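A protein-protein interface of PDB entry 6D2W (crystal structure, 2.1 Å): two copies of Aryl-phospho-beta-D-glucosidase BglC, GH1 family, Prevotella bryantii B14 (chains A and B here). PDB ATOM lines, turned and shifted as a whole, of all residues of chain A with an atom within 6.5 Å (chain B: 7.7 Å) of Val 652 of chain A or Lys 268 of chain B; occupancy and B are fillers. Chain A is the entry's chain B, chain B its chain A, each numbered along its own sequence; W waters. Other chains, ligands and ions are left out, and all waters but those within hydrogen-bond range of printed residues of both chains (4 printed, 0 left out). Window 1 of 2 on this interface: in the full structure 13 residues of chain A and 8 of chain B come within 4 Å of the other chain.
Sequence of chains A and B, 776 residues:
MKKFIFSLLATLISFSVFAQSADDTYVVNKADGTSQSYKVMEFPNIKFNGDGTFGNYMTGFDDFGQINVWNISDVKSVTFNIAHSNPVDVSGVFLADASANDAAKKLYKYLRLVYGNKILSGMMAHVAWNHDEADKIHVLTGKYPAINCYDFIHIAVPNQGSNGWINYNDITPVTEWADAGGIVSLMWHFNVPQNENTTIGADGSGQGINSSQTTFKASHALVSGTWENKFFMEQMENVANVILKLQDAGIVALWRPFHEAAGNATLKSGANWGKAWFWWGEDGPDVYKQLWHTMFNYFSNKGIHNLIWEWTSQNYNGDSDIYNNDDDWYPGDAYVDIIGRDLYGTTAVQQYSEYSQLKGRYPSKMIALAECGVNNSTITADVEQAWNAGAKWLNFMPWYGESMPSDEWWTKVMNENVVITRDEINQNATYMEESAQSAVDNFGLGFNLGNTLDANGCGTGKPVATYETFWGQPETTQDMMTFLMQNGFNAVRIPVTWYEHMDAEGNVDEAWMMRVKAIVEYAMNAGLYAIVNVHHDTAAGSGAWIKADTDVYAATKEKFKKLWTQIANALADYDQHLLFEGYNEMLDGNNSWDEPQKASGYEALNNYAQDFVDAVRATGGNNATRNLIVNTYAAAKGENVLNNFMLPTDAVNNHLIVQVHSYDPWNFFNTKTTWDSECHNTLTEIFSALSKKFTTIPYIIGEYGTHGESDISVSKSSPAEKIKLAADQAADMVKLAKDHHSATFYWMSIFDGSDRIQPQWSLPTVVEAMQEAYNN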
ATOM      1  N   TYR A 431       2.757 -22.983 -28.167  1.00  0.00           N
ATOM      2  CA  TYR A 431       1.326 -22.750 -28.289  1.00  0.00           C
ATOM      3  C   TYR A 431       0.959 -21.560 -27.415  1.00  0.00           C
ATOM      4  O   TYR A 431       1.531 -21.361 -26.340  1.00  0.00           O
ATOM      5  CB  TYR A 431       0.519 -23.988 -27.873  1.00  0.00           C
ATOM      6  CG  TYR A 431      -0.984 -23.797 -27.839  1.00  0.00           C
ATOM      7  CD1 TYR A 431      -1.626 -23.357 -26.688  1.00  0.00           C
ATOM      8  CD2 TYR A 431      -1.761 -24.084 -28.951  1.00  0.00           C
ATOM      9  CE1 TYR A 431      -2.999 -23.188 -26.657  1.00  0.00           C
ATOM     10  CE2 TYR A 431      -3.126 -23.923 -28.929  1.00  0.00           C
ATOM     11  CZ  TYR A 431      -3.743 -23.477 -27.782  1.00  0.00           C
ATOM     12  OH  TYR A 431      -5.110 -23.318 -27.771  1.00  0.00           O
ATOM     13  N   GLU A 433      -2.733 -19.542 -26.369  1.00  0.00           N
ATOM     14  CA  GLU A 433      -4.185 -19.517 -26.543  1.00  0.00           C
ATOM     15  C   GLU A 433      -4.616 -18.211 -27.199  1.00  0.00           C
ATOM     16  O   GLU A 433      -4.052 -17.145 -26.920  1.00  0.00           O
ATOM     17  CB  GLU A 433      -4.882 -19.705 -25.185  1.00  0.00           C
ATOM     18  CG  GLU A 433      -6.174 -18.881 -24.995  1.00  0.00           C
ATOM     19  CD  GLU A 433      -6.853 -19.077 -23.629  1.00  0.00           C
ATOM     20  OE1 GLU A 433      -7.284 -20.205 -23.300  1.00  0.00           O
ATOM     21  OE2 GLU A 433      -6.988 -18.079 -22.895  1.00  0.00           O
ATOM     22  N   ARG A 617     -12.084 -31.555 -26.143  1.00  0.00           N
ATOM     23  CA  ARG A 617     -11.555 -31.015 -24.895  1.00  0.00           C
ATOM     24  C   ARG A 617     -11.048 -32.122 -23.982  1.00  0.00           C
ATOM     25  O   ARG A 617     -10.122 -31.898 -23.197  1.00  0.00           O
ATOM     26  CB  ARG A 617     -12.616 -30.180 -24.175  1.00  0.00           C
ATOM     27  CG  ARG A 617     -13.126 -28.976 -24.975  1.00  0.00           C
ATOM     28  CD  ARG A 617     -12.093 -27.875 -25.077  1.00  0.00           C
ATOM     29  NE  ARG A 617     -12.653 -26.677 -25.695  1.00  0.00           N
ATOM     30  CZ  ARG A 617     -12.080 -26.012 -26.691  1.00  0.00           C
ATOM     31  NH1 ARG A 617     -10.920 -26.428 -27.184  1.00  0.00           N
ATOM     32  NH2 ARG A 617     -12.664 -24.928 -27.191  1.00  0.00           N
ATOM     33  N   GLY A 621      -4.136 -30.972 -23.274  1.00  0.00           N
ATOM     34  CA  GLY A 621      -3.032 -30.335 -23.979  1.00  0.00           C
ATOM     35  C   GLY A 621      -3.456 -29.029 -24.626  1.00  0.00           C
ATOM     36  O   GLY A 621      -4.202 -28.233 -24.045  1.00  0.00           O
ATOM     37  N   ASN A 622      -2.970 -28.806 -25.853  1.00  0.00           N
ATOM     38  CA  ASN A 622      -3.397 -27.656 -26.651  1.00  0.00           C
ATOM     39  C   ASN A 622      -4.891 -27.711 -26.960  1.00  0.00           C
ATOM     40  O   ASN A 622      -5.528 -26.668 -27.149  1.00  0.00           O
ATOM     41  CB  ASN A 622      -2.610 -27.592 -27.969  1.00  0.00           C
ATOM     42  CG  ASN A 622      -1.116 -27.298 -27.776  1.00  0.00           C
ATOM     43  OD1 ASN A 622      -0.670 -27.044 -26.657  1.00  0.00           O
ATOM     44  ND2 ASN A 622      -0.350 -27.346 -28.852  1.00  0.00           N
ATOM     45  N   ALA A 624      -7.278 -28.257 -25.083  1.00  0.00           N
ATOM     46  CA  ALA A 624      -8.107 -27.656 -24.044  1.00  0.00           C
ATOM     47  C   ALA A 624      -8.576 -26.253 -24.423  1.00  0.00           C
ATOM     48  O   ALA A 624      -9.631 -25.811 -23.957  1.00  0.00           O
ATOM     49  CB  ALA A 624      -7.352 -27.606 -22.718  1.00  0.00           C
ATOM     50  N   THR A 625      -7.805 -25.527 -25.234  1.00  0.00           N
ATOM     51  CA  THR A 625      -8.177 -24.169 -25.605  1.00  0.00           C
ATOM     52  C   THR A 625      -8.187 -23.915 -27.110  1.00  0.00           C
ATOM     53  O   THR A 625      -8.429 -22.774 -27.522  1.00  0.00           O
ATOM     54  CB  THR A 625      -7.239 -23.156 -24.934  1.00  0.00           C
ATOM     55  OG1 THR A 625      -5.892 -23.418 -25.335  1.00  0.00           O
ATOM     56  CG2 THR A 625      -7.337 -23.271 -23.418  1.00  0.00           C
ATOM     57  N   ARG A 626      -7.928 -24.928 -27.934  1.00  0.00           N
ATOM     58  CA  ARG A 626      -8.000 -24.752 -29.377  1.00  0.00           C
ATOM     59  C   ARG A 626      -9.379 -24.238 -29.777  1.00  0.00           C
ATOM     60  O   ARG A 626     -10.401 -24.647 -29.225  1.00  0.00           O
ATOM     61  CB  ARG A 626      -7.703 -26.070 -30.094  1.00  0.00           C
ATOM     62  CG  ARG A 626      -7.857 -26.004 -31.602  1.00  0.00           C
ATOM     63  CD  ARG A 626      -7.393 -27.280 -32.302  1.00  0.00           C
ATOM     64  NE  ARG A 626      -6.327 -27.971 -31.581  1.00  0.00           N
ATOM     65  CZ  ARG A 626      -5.031 -27.719 -31.747  1.00  0.00           C
ATOM     66  NH1 ARG A 626      -4.637 -26.788 -32.603  1.00  0.00           N
ATOM     67  NH2 ARG A 626      -4.127 -28.391 -31.053  1.00  0.00           N
ATOM     68  N   THR A 649     -21.811 -26.117 -24.686  1.00  0.00           N
ATOM     69  CA  THR A 649     -21.208 -25.652 -23.447  1.00  0.00           C
ATOM     70  C   THR A 649     -19.728 -26.021 -23.416  1.00  0.00           C
ATOM     71  O   THR A 649     -19.360 -27.170 -23.671  1.00  0.00           O
ATOM     72  CB  THR A 649     -21.937 -26.267 -22.252  1.00  0.00           C
ATOM     73  OG1 THR A 649     -23.261 -25.724 -22.173  1.00  0.00           O
ATOM     74  CG2 THR A 649     -21.199 -25.967 -20.967  1.00  0.00           C
ATOM     75  N   ASP A 650     -18.882 -25.042 -23.096  1.00  0.00           N
ATOM     76  CA  ASP A 650     -17.434 -25.191 -23.107  1.00  0.00           C
ATOM     77  C   ASP A 650     -16.892 -24.789 -21.741  1.00  0.00           C
ATOM     78  O   ASP A 650     -17.349 -23.803 -21.154  1.00  0.00           O
ATOM     79  CB  ASP A 650     -16.819 -24.315 -24.219  1.00  0.00           C
ATOM     80  CG  ASP A 650     -15.532 -24.894 -24.807  1.00  0.00           C
ATOM     81  OD1 ASP A 650     -15.046 -25.945 -24.328  1.00  0.00           O
ATOM     82  OD2 ASP A 650     -14.999 -24.272 -25.759  1.00  0.00           O
ATOM     83  N   ALA A 651     -15.925 -25.558 -21.226  1.00  0.00           N
ATOM     84  CA  ALA A 651     -15.321 -25.214 -19.940  1.00  0.00           C
ATOM     85  C   ALA A 651     -14.412 -23.996 -20.030  1.00  0.00           C
ATOM     86  O   ALA A 651     -14.201 -23.318 -19.018  1.00  0.00           O
ATOM     87  CB  ALA A 651     -14.530 -26.396 -19.379  1.00  0.00           C
ATOM     88  N   VAL A 652     -13.872 -23.709 -21.209  1.00  0.00           N
ATOM     89  CA  VAL A 652     -13.073 -22.521 -21.431  1.00  0.00           C
ATOM     90  C   VAL A 652     -13.927 -21.489 -22.157  1.00  0.00           C
ATOM     91  O   VAL A 652     -14.980 -21.792 -22.727  1.00  0.00           O
ATOM     92  CB  VAL A 652     -11.784 -22.835 -22.217  1.00  0.00           C
ATOM     93  CG1 VAL A 652     -10.885 -23.727 -21.389  1.00  0.00           C
ATOM     94  CG2 VAL A 652     -12.114 -23.494 -23.553  1.00  0.00           C
ATOM     95  N   ASN A 653     -13.466 -20.245 -22.141  1.00  0.00           N
ATOM     96  CA  ASN A 653     -14.250 -19.127 -22.635  1.00  0.00           C
ATOM     97  C   ASN A 653     -13.712 -18.611 -23.964  1.00  0.00           C
ATOM     98  O   ASN A 653     -12.495 -18.543 -24.171  1.00  0.00           O
ATOM     99  CB  ASN A 653     -14.271 -17.992 -21.615  1.00  0.00           C
ATOM    100  CG  ASN A 653     -15.566 -17.220 -21.653  1.00  0.00           C
ATOM    101  OD1 ASN A 653     -16.288 -17.246 -22.656  1.00  0.00           O
ATOM    102  ND2 ASN A 653     -15.879 -16.535 -20.562  1.00  0.00           N
ATOM    103  N   ASN A 654     -14.644 -18.249 -24.855  1.00  0.00           N
ATOM    104  CA  ASN A 654     -14.347 -17.583 -26.122  1.00  0.00           C
ATOM    105  C   ASN A 654     -13.451 -18.433 -27.015  1.00  0.00           C
ATOM    106  O   ASN A 654     -12.471 -17.951 -27.586  1.00  0.00           O
ATOM    107  CB  ASN A 654     -13.726 -16.204 -25.893  1.00  0.00           C
ATOM    108  CG  ASN A 654     -14.533 -15.349 -24.935  1.00  0.00           C
ATOM    109  OD1 ASN A 654     -14.098 -15.060 -23.823  1.00  0.00           O
ATOM    110  ND2 ASN A 654     -15.721 -14.938 -25.368  1.00  0.00           N
ATOM    111  N   HIS A 655     -13.809 -19.706 -27.169  1.00  0.00           N
ATOM    112  CA  HIS A 655     -13.055 -20.558 -28.084  1.00  0.00           C
ATOM    113  C   HIS A 655     -13.972 -21.340 -29.017  1.00  0.00           C
ATOM    114  O   HIS A 655     -13.624 -22.440 -29.463  1.00  0.00           O
ATOM    115  CB  HIS A 655     -12.120 -21.496 -27.318  1.00  0.00           C
ATOM    116  CG  HIS A 655     -11.015 -20.776 -26.605  1.00  0.00           C
ATOM    117  ND1 HIS A 655     -10.110 -19.968 -27.261  1.00  0.00           N
ATOM    118  CD2 HIS A 655     -10.672 -20.735 -25.295  1.00  0.00           C
ATOM    119  CE1 HIS A 655      -9.260 -19.459 -26.387  1.00  0.00           C
ATOM    120  NE2 HIS A 655      -9.574 -19.914 -25.187  1.00  0.00           N
ATOM    121  N   LEU A 656     -15.135 -20.772 -29.335  1.00  0.00           N
ATOM    122  CA  LEU A 656     -16.073 -21.352 -30.283  1.00  0.00           C
ATOM    123  C   LEU A 656     -16.378 -20.352 -31.388  1.00  0.00           C
ATOM    124  O   LEU A 656     -16.472 -19.145 -31.144  1.00  0.00           O
ATOM    125  CB  LEU A 656     -17.373 -21.780 -29.598  1.00  0.00           C
ATOM    126  CG  LEU A 656     -17.260 -22.908 -28.569  1.00  0.00           C
ATOM    127  CD1 LEU A 656     -18.625 -23.187 -27.954  1.00  0.00           C
ATOM    128  CD2 LEU A 656     -16.674 -24.176 -29.188  1.00  0.00           C
ATOM    129  N   ASN B 264       2.814 -25.080 -11.625  1.00  0.00           N
ATOM    130  CA  ASN B 264       1.704 -24.447 -12.325  1.00  0.00           C
ATOM    131  C   ASN B 264       1.869 -24.497 -13.840  1.00  0.00           C
ATOM    132  O   ASN B 264       1.179 -23.763 -14.558  1.00  0.00           O
ATOM    133  CB  ASN B 264       1.546 -22.995 -11.866  1.00  0.00           C
ATOM    134  CG  ASN B 264       0.858 -22.883 -10.528  1.00  0.00           C
ATOM    135  OD1 ASN B 264      -0.005 -23.694 -10.193  1.00  0.00           O
ATOM    136  ND2 ASN B 264       1.239 -21.877  -9.749  1.00  0.00           N
ATOM    137  N   ALA B 265       2.767 -25.351 -14.341  1.00  0.00           N
ATOM    138  CA  ALA B 265       3.054 -25.388 -15.770  1.00  0.00           C
ATOM    139  C   ALA B 265       1.918 -25.975 -16.602  1.00  0.00           C
ATOM    140  O   ALA B 265       2.004 -25.930 -17.831  1.00  0.00           O
ATOM    141  CB  ALA B 265       4.339 -26.183 -16.033  1.00  0.00           C
ATOM    142  N   THR B 266       0.881 -26.537 -15.982  1.00  0.00           N
ATOM    143  CA  THR B 266      -0.243 -27.110 -16.716  1.00  0.00           C
ATOM    144  C   THR B 266      -1.339 -26.095 -16.981  1.00  0.00           C
ATOM    145  O   THR B 266      -2.455 -26.484 -17.343  1.00  0.00           O
ATOM    146  CB  THR B 266      -0.841 -28.292 -15.953  1.00  0.00           C
ATOM    147  OG1 THR B 266      -1.134 -27.882 -14.616  1.00  0.00           O
ATOM    148  CG2 THR B 266       0.126 -29.451 -15.921  1.00  0.00           C
ATOM    149  N   LEU B 267      -1.050 -24.813 -16.778  1.00  0.00           N
ATOM    150  CA  LEU B 267      -2.022 -23.759 -17.016  1.00  0.00           C
ATOM    151  C   LEU B 267      -2.490 -23.795 -18.464  1.00  0.00           C
ATOM    152  O   LEU B 267      -1.677 -23.886 -19.389  1.00  0.00           O
ATOM    153  CB  LEU B 267      -1.389 -22.407 -16.684  1.00  0.00           C
ATOM    154  CG  LEU B 267      -2.288 -21.184 -16.554  1.00  0.00           C
ATOM    155  CD1 LEU B 267      -3.251 -21.316 -15.381  1.00  0.00           C
ATOM    156  CD2 LEU B 267      -1.432 -19.940 -16.419  1.00  0.00           C
ATOM    157  N   LYS B 268      -3.812 -23.731 -18.658  1.00  0.00           N
ATOM    158  CA  LYS B 268      -4.372 -23.916 -19.993  1.00  0.00           C
ATOM    159  C   LYS B 268      -3.916 -22.823 -20.951  1.00  0.00           C
ATOM    160  O   LYS B 268      -3.698 -23.082 -22.139  1.00  0.00           O
ATOM    161  CB  LYS B 268      -5.898 -23.947 -19.929  1.00  0.00           C
ATOM    162  CG  LYS B 268      -6.498 -25.193 -19.294  1.00  0.00           C
ATOM    163  CD  LYS B 268      -7.997 -25.195 -19.508  1.00  0.00           C
ATOM    164  CE  LYS B 268      -8.660 -26.360 -18.816  1.00  0.00           C
ATOM    165  NZ  LYS B 268     -10.131 -26.259 -18.971  1.00  0.00           N
ATOM    166  N   SER B 269      -3.771 -21.595 -20.453  1.00  0.00           N
ATOM    167  CA  SER B 269      -3.534 -20.462 -21.343  1.00  0.00           C
ATOM    168  C   SER B 269      -2.118 -20.485 -21.909  1.00  0.00           C
ATOM    169  O   SER B 269      -1.917 -20.301 -23.117  1.00  0.00           O
ATOM    170  CB  SER B 269      -3.793 -19.155 -20.599  1.00  0.00           C
ATOM    171  OG  SER B 269      -2.950 -19.056 -19.467  1.00  0.00           O
ATOM    172  N   GLY B 270      -1.124 -20.708 -21.050  1.00  0.00           N
ATOM    173  CA  GLY B 270       0.271 -20.650 -21.438  1.00  0.00           C
ATOM    174  C   GLY B 270       1.029 -19.456 -20.898  1.00  0.00           C
ATOM    175  O   GLY B 270       2.219 -19.314 -21.204  1.00  0.00           O
ATOM    176  N   ALA B 271       0.381 -18.589 -20.119  1.00  0.00           N
ATOM    177  CA  ALA B 271       1.075 -17.477 -19.485  1.00  0.00           C
ATOM    178  C   ALA B 271       2.123 -18.001 -18.513  1.00  0.00           C
ATOM    179  O   ALA B 271       1.867 -18.933 -17.747  1.00  0.00           O
ATOM    180  CB  ALA B 271       0.077 -16.577 -18.753  1.00  0.00           C
ATOM    181  N   TYR B 316      -5.351 -31.056 -10.815  1.00  0.00           N
ATOM    182  CA  TYR B 316      -5.759 -29.864 -11.551  1.00  0.00           C
ATOM    183  C   TYR B 316      -5.381 -28.576 -10.830  1.00  0.00           C
ATOM    184  O   TYR B 316      -5.936 -27.514 -11.138  1.00  0.00           O
ATOM    185  CB  TYR B 316      -7.266 -29.876 -11.819  1.00  0.00           C
ATOM    186  CG  TYR B 316      -7.721 -30.962 -12.772  1.00  0.00           C
ATOM    187  CD1 TYR B 316      -7.607 -30.804 -14.149  1.00  0.00           C
ATOM    188  CD2 TYR B 316      -8.282 -32.140 -12.289  1.00  0.00           C
ATOM    189  CE1 TYR B 316      -8.038 -31.799 -15.025  1.00  0.00           C
ATOM    190  CE2 TYR B 316      -8.709 -33.139 -13.151  1.00  0.00           C
ATOM    191  CZ  TYR B 316      -8.584 -32.966 -14.515  1.00  0.00           C
ATOM    192  OH  TYR B 316      -9.006 -33.968 -15.358  1.00  0.00           O
ATOM    193  N   ASP B 319      -8.255 -26.329  -9.710  1.00  0.00           N
ATOM    194  CA  ASP B 319      -9.155 -25.585 -10.603  1.00  0.00           C
ATOM    195  C   ASP B 319      -9.013 -26.123 -12.035  1.00  0.00           C
ATOM    196  O   ASP B 319      -8.201 -25.625 -12.815  1.00  0.00           O
ATOM    197  CB  ASP B 319      -8.873 -24.101 -10.549  1.00  0.00           C
ATOM    198  CG  ASP B 319      -9.980 -23.274 -11.189  1.00  0.00           C
ATOM    199  OD1 ASP B 319     -10.807 -23.851 -11.931  1.00  0.00           O
ATOM    200  OD2 ASP B 319     -10.026 -22.047 -10.947  1.00  0.00           O
ATOM    201  N   SER B 320      -9.837 -27.117 -12.368  1.00  0.00           N
ATOM    202  CA  SER B 320      -9.793 -27.717 -13.699  1.00  0.00           C
ATOM    203  C   SER B 320     -10.276 -26.773 -14.793  1.00  0.00           C
ATOM    204  O   SER B 320     -10.047 -27.056 -15.974  1.00  0.00           O
ATOM    205  CB  SER B 320     -10.627 -29.001 -13.730  1.00  0.00           C
ATOM    206  OG  SER B 320     -12.006 -28.723 -13.558  1.00  0.00           O
ATOM    207  N   ASP B 321     -10.935 -25.669 -14.441  1.00  0.00           N
ATOM    208  CA  ASP B 321     -11.366 -24.726 -15.465  1.00  0.00           C
ATOM    209  C   ASP B 321     -10.184 -24.004 -16.095  1.00  0.00           C
ATOM    210  O   ASP B 321     -10.257 -23.601 -17.261  1.00  0.00           O
ATOM    211  CB  ASP B 321     -12.349 -23.719 -14.875  1.00  0.00           C
ATOM    212  CG  ASP B 321     -13.754 -24.275 -14.772  1.00  0.00           C
ATOM    213  OD1 ASP B 321     -14.008 -25.356 -15.346  1.00  0.00           O
ATOM    214  OD2 ASP B 321     -14.605 -23.634 -14.117  1.00  0.00           O
ATOM    215  N   ILE B 322      -9.086 -23.847 -15.364  1.00  0.00           N
ATOM    216  CA  ILE B 322      -7.933 -23.115 -15.874  1.00  0.00           C
ATOM    217  C   ILE B 322      -6.681 -23.971 -15.993  1.00  0.00           C
ATOM    218  O   ILE B 322      -5.696 -23.508 -16.584  1.00  0.00           O
ATOM    219  CB  ILE B 322      -7.640 -21.862 -15.022  1.00  0.00           C
ATOM    220  CG1 ILE B 322      -7.185 -22.266 -13.626  1.00  0.00           C
ATOM    221  CG2 ILE B 322      -8.882 -20.968 -14.940  1.00  0.00           C
ATOM    222  CD1 ILE B 322      -6.567 -21.133 -12.849  1.00  0.00           C
ATOM    223  N   TYR B 323      -6.679 -25.197 -15.478  1.00  0.00           N
ATOM    224  CA  TYR B 323      -5.513 -26.069 -15.541  1.00  0.00           C
ATOM    225  C   TYR B 323      -5.856 -27.360 -16.268  1.00  0.00           C
ATOM    226  O   TYR B 323      -6.947 -27.910 -16.096  1.00  0.00           O
ATOM    227  CB  TYR B 323      -4.988 -26.426 -14.139  1.00  0.00           C
ATOM    228  CG  TYR B 323      -4.300 -25.303 -13.398  1.00  0.00           C
ATOM    229  CD1 TYR B 323      -2.993 -24.951 -13.697  1.00  0.00           C
ATOM    230  CD2 TYR B 323      -4.956 -24.603 -12.391  1.00  0.00           C
ATOM    231  CE1 TYR B 323      -2.357 -23.934 -13.023  1.00  0.00           C
ATOM    232  CE2 TYR B 323      -4.328 -23.573 -11.708  1.00  0.00           C
ATOM    233  CZ  TYR B 323      -3.025 -23.247 -12.032  1.00  0.00           C
ATOM    234  OH  TYR B 323      -2.374 -22.237 -11.369  1.00  0.00           O
ATOM    235  N   ASN B 324      -4.922 -27.835 -17.086  1.00  0.00           N
ATOM    236  CA  ASN B 324      -4.924 -29.235 -17.470  1.00  0.00           C
ATOM    237  C   ASN B 324      -4.444 -30.075 -16.294  1.00  0.00           C
ATOM    238  O   ASN B 324      -3.781 -29.579 -15.381  1.00  0.00           O
ATOM    239  CB  ASN B 324      -4.013 -29.472 -18.675  1.00  0.00           C
ATOM    240  CG  ASN B 324      -4.618 -28.986 -19.976  1.00  0.00           C
ATOM    241  OD1 ASN B 324      -5.766 -29.294 -20.292  1.00  0.00           O
ATOM    242  ND2 ASN B 324      -3.844 -28.225 -20.744  1.00  0.00           N
ATOM    243  N   ASN B 325      -4.778 -31.360 -16.314  1.00  0.00           N
ATOM    244  CA  ASN B 325      -4.146 -32.227 -15.335  1.00  0.00           C
ATOM    245  C   ASN B 325      -2.717 -32.534 -15.788  1.00  0.00           C
ATOM    246  O   ASN B 325      -2.299 -32.160 -16.887  1.00  0.00           O
ATOM    247  CB  ASN B 325      -4.975 -33.497 -15.110  1.00  0.00           C
ATOM    248  CG  ASN B 325      -5.044 -34.393 -16.335  1.00  0.00           C
ATOM    249  OD1 ASN B 325      -4.045 -34.627 -17.005  1.00  0.00           O
ATOM    250  ND2 ASN B 325      -6.237 -34.911 -16.625  1.00  0.00           N
HETATM  251  O   HOH W   1      -4.754 -25.343 -23.549  1.00  0.00           O
HETATM  252  O   HOH W   2     -11.747 -21.512 -18.087  1.00  0.00           O
HETATM  253  O   HOH W   3     -10.878 -27.068 -21.730  1.00  0.00           O
HETATM  254  O   HOH W   4       2.224 -19.057 -24.581  1.00  0.00           O
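N of Glu 433 of chain A lies within hydrogen-bond range of O of Ser 269 of chain B (3.4 Å).
O of Gly 621 of chain A lies within hydrogen-bond range of ND2 of Asn 324 of chain B, 3.3 Å away.
O of Ser 320 of chain B lies within hydrogen-bond range of NZ of Lys 268 of chain B (3.1 Å).
O of Ile 322 of chain B sits at hydrogen-bond distance from N of Lys 268 of chain B (2.8 Å).
The side-chain hydroxyl of Ser 269 of chain B sits at hydrogen-bond distance from the backbone NH of Ala 271 of chain B.
The side-chain hydroxyl (OH) of Tyr 431 of chain A is in hydrogen-bond range of the side-chain hydroxyl (OG1) of Thr 625 of chain A (2.6 Å).
A ring nitrogen (NE2) of His 655 of chain A sits at hydrogen-bond distance from the side-chain carboxylate (OE1) of Glu 433 of chain A (3.0 Å).
A ring nitrogen (ND1) of His 655 of chain A lies within hydrogen-bond range of the backbone carbonyl oxygen (O) of Thr 625 of chain A, at 3.3 Å.
Asn 324 of chain B touches Ala 624 of chain A (OD1 to CB, 3.4 Å).
Lys 268 of chain B touches Thr 625 of chain A.
Val 652 of chain A touches Lys 268 of chain B.
Val 652 of chain A touches one residue of chain B.
Lys 268 of chain B touches just these residues of chain A: Thr 625 and Val 652.
No residue of chain B comes within 4 Å of Ala 651 of chain A.
Of the printed residues of chain B, Thr 625 of chain A touches Lys 268.
Printed residues of chain B within 4 Å of Glu 433 of chain A: Ser 269.
Printed residues of chain B within 4 Å of Gly 621 of chain A: Asn 324.
Of the printed residues of chain A, Asn 324 of chain B touches Gly 621 and Ala 624.
Printed residues of chain A within 4 Å of Ser 269 of chain B: Glu 433.
The nearest residue of chain B that does not touch Val 652 of chain A is Asp 321 of chain B (4.2 Å).
The nearest residue of chain A that does not touch Lys 268 of chain B is Ala 624 of chain A (4.1 Å).
The nearest printed residue of chain B that does not touch Thr 625 of chain A is Ser 269 of chain B (4.9 Å).
Printed residues of chain A that touch a printed residue of chain B: Glu 433, Gly 621, Ala 624, Thr 625 and Val 652.
Hydrophobic or aromatic side chains of chain A that line the printed part of chain B: Ala 624 and Val 652.
No position is printed for both chains.
Of the 5 pairs that touch across the chains among the printed residues, none has its exchanged pair printed and touching as well.
Water W2 bridges the backbone carbonyl oxygen of Asp 321 of chain B (2.7 Å) and the backbone carbonyl oxygen of Ala 651 of chain A (3.2 Å).
Water W3 lies within hydrogen-bond range of the backbone carbonyl oxygen (O) of Ala 624 of chain A (2.8 Å) and the side-chain amino group (NZ) of Lys 268 of chain B (3.0 Å).
Water W1 lies within hydrogen-bond range of OG1 of Thr 625 of chain A, O of Lys 268 of chain B and O of Gly 621 of chain A.
Water W4 lies within hydrogen-bond range of O of Tyr 431 of chain A (3.0 Å) and O of Gly 270 of chain B (3.4 Å).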
